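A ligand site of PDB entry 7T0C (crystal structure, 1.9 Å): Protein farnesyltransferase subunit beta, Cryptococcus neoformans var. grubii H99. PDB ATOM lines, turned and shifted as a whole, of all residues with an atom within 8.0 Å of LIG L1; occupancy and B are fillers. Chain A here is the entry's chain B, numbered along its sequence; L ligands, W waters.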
ATOM      1  N   LEU A  50     -30.592  14.946 -20.758  1.00  0.00           N
ATOM      2  CA  LEU A  50     -31.307  13.764 -20.204  1.00  0.00           C
ATOM      3  C   LEU A  50     -31.463  12.654 -21.249  1.00  0.00           C
ATOM      4  O   LEU A  50     -31.355  11.485 -20.889  1.00  0.00           O
ATOM      5  CB  LEU A  50     -32.692  14.235 -19.769  1.00  0.00           C
ATOM      6  CG  LEU A  50     -33.074  14.007 -18.312  1.00  0.00           C
ATOM      7  CD1 LEU A  50     -34.552  13.670 -18.178  1.00  0.00           C
ATOM      8  CD2 LEU A  50     -32.221  12.916 -17.707  1.00  0.00           C
ATOM      9  N   TYR A  58     -22.370  11.028 -29.683  1.00  0.00           N
ATOM     10  CA  TYR A  58     -22.482  10.831 -28.249  1.00  0.00           C
ATOM     11  C   TYR A  58     -21.105  10.975 -27.589  1.00  0.00           C
ATOM     12  O   TYR A  58     -20.125  10.389 -28.061  1.00  0.00           O
ATOM     13  CB  TYR A  58     -23.085   9.462 -27.928  1.00  0.00           C
ATOM     14  CG  TYR A  58     -23.185   9.200 -26.447  1.00  0.00           C
ATOM     15  CD1 TYR A  58     -22.495   8.151 -25.845  1.00  0.00           C
ATOM     16  CD2 TYR A  58     -23.954  10.029 -25.630  1.00  0.00           C
ATOM     17  CE1 TYR A  58     -22.567   7.932 -24.469  1.00  0.00           C
ATOM     18  CE2 TYR A  58     -24.050   9.817 -24.270  1.00  0.00           C
ATOM     19  CZ  TYR A  58     -23.347   8.783 -23.681  1.00  0.00           C
ATOM     20  OH  TYR A  58     -23.442   8.585 -22.321  1.00  0.00           O
ATOM     21  N   GLY A  60     -20.056  10.223 -24.387  1.00  0.00           N
ATOM     22  CA  GLY A  60     -19.643   9.374 -23.292  1.00  0.00           C
ATOM     23  C   GLY A  60     -18.194   8.905 -23.382  1.00  0.00           C
ATOM     24  O   GLY A  60     -17.680   8.692 -24.482  1.00  0.00           O
ATOM     25  N   LEU A  61     -17.540   8.753 -22.234  1.00  0.00           N
ATOM     26  CA  LEU A  61     -16.137   8.356 -22.185  1.00  0.00           C
ATOM     27  C   LEU A  61     -15.984   6.937 -22.708  1.00  0.00           C
ATOM     28  O   LEU A  61     -16.552   5.996 -22.153  1.00  0.00           O
ATOM     29  CB  LEU A  61     -15.613   8.448 -20.759  1.00  0.00           C
ATOM     30  CG  LEU A  61     -14.094   8.214 -20.574  1.00  0.00           C
ATOM     31  CD1 LEU A  61     -13.281   9.329 -21.257  1.00  0.00           C
ATOM     32  CD2 LEU A  61     -13.761   8.124 -19.079  1.00  0.00           C
ATOM     33  N   ILE A 486     -19.895  14.636 -11.954  1.00  0.00           N
ATOM     34  CA  ILE A 486     -19.608  13.732 -13.068  1.00  0.00           C
ATOM     35  C   ILE A 486     -20.443  14.190 -14.263  1.00  0.00           C
ATOM     36  O   ILE A 486     -21.597  13.784 -14.416  1.00  0.00           O
ATOM     37  CB  ILE A 486     -19.865  12.255 -12.745  1.00  0.00           C
ATOM     38  CG1 ILE A 486     -19.271  11.877 -11.378  1.00  0.00           C
ATOM     39  CG2 ILE A 486     -19.257  11.365 -13.830  1.00  0.00           C
ATOM     40  CD1 ILE A 486     -17.736  12.146 -11.269  1.00  0.00           C
ATOM     41  N   VAL A 487     -19.844  15.019 -15.128  1.00  0.00           N
ATOM     42  CA  VAL A 487     -20.554  15.492 -16.312  1.00  0.00           C
ATOM     43  C   VAL A 487     -20.922  14.298 -17.183  1.00  0.00           C
ATOM     44  O   VAL A 487     -20.093  13.420 -17.442  1.00  0.00           O
ATOM     45  CB  VAL A 487     -19.701  16.521 -17.074  1.00  0.00           C
ATOM     46  CG1 VAL A 487     -20.327  16.829 -18.447  1.00  0.00           C
ATOM     47  CG2 VAL A 487     -19.545  17.789 -16.249  1.00  0.00           C
ATOM     48  N   GLY A 488     -22.181  14.268 -17.637  1.00  0.00           N
ATOM     49  CA  GLY A 488     -22.649  13.248 -18.559  1.00  0.00           C
ATOM     50  C   GLY A 488     -23.163  11.965 -17.928  1.00  0.00           C
ATOM     51  O   GLY A 488     -23.588  11.062 -18.663  1.00  0.00           O
ATOM     52  N   GLY A 489     -23.125  11.839 -16.608  1.00  0.00           N
ATOM     53  CA  GLY A 489     -23.636  10.661 -15.945  1.00  0.00           C
ATOM     54  C   GLY A 489     -22.530   9.813 -15.358  1.00  0.00           C
ATOM     55  O   GLY A 489     -21.355   9.918 -15.740  1.00  0.00           O
ATOM     56  N   LYS A 490     -22.921   8.932 -14.436  1.00  0.00           N
ATOM     57  CA  LYS A 490     -21.944   8.251 -13.582  1.00  0.00           C
ATOM     58  C   LYS A 490     -21.085   7.233 -14.325  1.00  0.00           C
ATOM     59  O   LYS A 490     -20.010   6.876 -13.836  1.00  0.00           O
ATOM     60  CB  LYS A 490     -22.663   7.588 -12.401  1.00  0.00           C
ATOM     61  CG  LYS A 490     -23.116   8.585 -11.360  1.00  0.00           C
ATOM     62  CD  LYS A 490     -23.713   7.916 -10.138  1.00  0.00           C
ATOM     63  CE  LYS A 490     -24.223   8.951  -9.148  1.00  0.00           C
ATOM     64  NZ  LYS A 490     -25.313   8.386  -8.290  1.00  0.00           N
ATOM     65  N   ASP A 491     -21.515   6.767 -15.508  1.00  0.00           N
ATOM     66  CA  ASP A 491     -20.644   5.905 -16.312  1.00  0.00           C
ATOM     67  C   ASP A 491     -19.385   6.629 -16.789  1.00  0.00           C
ATOM     68  O   ASP A 491     -18.429   5.959 -17.208  1.00  0.00           O
ATOM     69  CB  ASP A 491     -21.410   5.326 -17.503  1.00  0.00           C
ATOM     70  CG  ASP A 491     -22.370   4.220 -17.110  1.00  0.00           C
ATOM     71  OD1 ASP A 491     -22.018   3.405 -16.227  1.00  0.00           O
ATOM     72  OD2 ASP A 491     -23.496   4.163 -17.668  1.00  0.00           O
ATOM     73  N   ASN A 492     -19.354   7.966 -16.743  1.00  0.00           N
ATOM     74  CA  ASN A 492     -18.138   8.684 -17.092  1.00  0.00           C
ATOM     75  C   ASN A 492     -17.155   8.800 -15.933  1.00  0.00           C
ATOM     76  O   ASN A 492     -16.041   9.296 -16.147  1.00  0.00           O
ATOM     77  CB  ASN A 492     -18.453  10.097 -17.607  1.00  0.00           C
ATOM     78  CG  ASN A 492     -19.105  10.109 -18.970  1.00  0.00           C
ATOM     79  OD1 ASN A 492     -19.002   9.148 -19.741  1.00  0.00           O
ATOM     80  ND2 ASN A 492     -19.804  11.198 -19.286  1.00  0.00           N
ATOM     81  N   ARG A 493     -17.534   8.398 -14.723  1.00  0.00           N
ATOM     82  CA  ARG A 493     -16.676   8.604 -13.562  1.00  0.00           C
ATOM     83  C   ARG A 493     -15.385   7.796 -13.693  1.00  0.00           C
ATOM     84  O   ARG A 493     -15.418   6.618 -14.060  1.00  0.00           O
ATOM     85  CB  ARG A 493     -17.410   8.210 -12.283  1.00  0.00           C
ATOM     86  CG  ARG A 493     -16.534   8.323 -11.036  1.00  0.00           C
ATOM     87  CD  ARG A 493     -16.973   7.358  -9.946  1.00  0.00           C
ATOM     88  NE  ARG A 493     -16.231   7.555  -8.706  1.00  0.00           N
ATOM     89  CZ  ARG A 493     -15.141   6.880  -8.346  1.00  0.00           C
ATOM     90  NH1 ARG A 493     -14.624   5.942  -9.143  1.00  0.00           N
ATOM     91  NH2 ARG A 493     -14.553   7.141  -7.191  1.00  0.00           N
HETATM   92  O1  LIG L   1     -26.038   6.757 -13.081  1.00  0.00           O
HETATM   93  O2  LIG L   1     -25.709   9.007 -14.002  1.00  0.00           O
HETATM   94  O3  LIG L   1     -24.656   6.439 -15.904  1.00  0.00           O
HETATM   95  O4  LIG L   1     -27.890   8.195 -13.265  1.00  0.00           O
HETATM   96  C1  LIG L   1     -25.408   3.691 -22.217  1.00  0.00           C
HETATM   97  C2  LIG L   1     -26.668   3.955 -21.400  1.00  0.00           C
HETATM   98  C3  LIG L   1     -24.483   4.923 -22.248  1.00  0.00           C
HETATM   99  C4  LIG L   1     -26.364   4.489 -19.993  1.00  0.00           C
HETATM  100  C5  LIG L   1     -24.124   5.370 -20.830  1.00  0.00           C
HETATM  101  C6  LIG L   1     -26.059   6.540 -17.894  1.00  0.00           C
HETATM  102  C7  LIG L   1     -26.976   7.337 -15.686  1.00  0.00           C
HETATM  103  N1  LIG L   1     -24.940   5.928 -18.602  1.00  0.00           N
HETATM  104  C8  LIG L   1     -25.984   6.376 -16.378  1.00  0.00           C
HETATM  105  C9  LIG L   1     -25.364   5.661 -19.986  1.00  0.00           C
HETATM  106  S1  LIG L   1     -26.624   7.824 -13.973  1.00  0.00           S
HETATM  107  O1  LG2 L   2     -17.397   2.173 -24.354  1.00  0.00           O
HETATM  108  O2  LG2 L   2     -15.267   2.181 -25.186  1.00  0.00           O
HETATM  109  O3  LG2 L   2     -17.813   1.111 -28.325  1.00  0.00           O
HETATM  110  O4  LG2 L   2     -17.077   3.004 -26.703  1.00  0.00           O
HETATM  111  C1  LG2 L   2     -21.488  -4.526 -29.130  1.00  0.00           C
HETATM  112  C2  LG2 L   2     -20.757  -4.202 -27.815  1.00  0.00           C
HETATM  113  C3  LG2 L   2     -21.865  -3.250 -29.900  1.00  0.00           C
HETATM  114  C4  LG2 L   2     -19.569  -3.256 -28.045  1.00  0.00           C
HETATM  115  C5  LG2 L   2     -20.711  -2.254 -30.042  1.00  0.00           C
HETATM  116  C6  LG2 L   2     -17.797  -1.242 -28.019  1.00  0.00           C
HETATM  117  C7  LG2 L   2     -16.976   0.264 -26.214  1.00  0.00           C
HETATM  118  N1  LG2 L   2     -18.904  -1.036 -28.930  1.00  0.00           N
HETATM  119  C8  LG2 L   2     -17.074   0.082 -27.731  1.00  0.00           C
HETATM  120  C9  LG2 L   2     -20.034  -1.956 -28.699  1.00  0.00           C
HETATM  121  S1  LG2 L   2     -16.680   1.973 -25.659  1.00  0.00           S
HETATM  122  O   HOH W   1     -30.867   8.049 -14.282  1.00  0.00           O
HETATM  123  O   HOH W   2     -23.146   8.195 -18.423  1.00  0.00           O
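Water W2 bridges N1 of LIG L1 (2.9 Å) and O of Gly 488 (2.9 Å).
Merely in contact with LIG L1: Gly 489 (3.3 Å) and Tyr 58 (3.6 Å).
The backbone NH (N) of Asp 491 sits at hydrogen-bond distance from an oxygen (O3) of LIG L1 (3.2 Å).
A nitrogen (N1) of LIG L1 lies within salt-bridge range of the side-chain carboxylate (OD2) of Asp 491, 2.5 Å away.
O2 of LIG L1 sits at hydrogen-bond distance from N of Lys 490.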
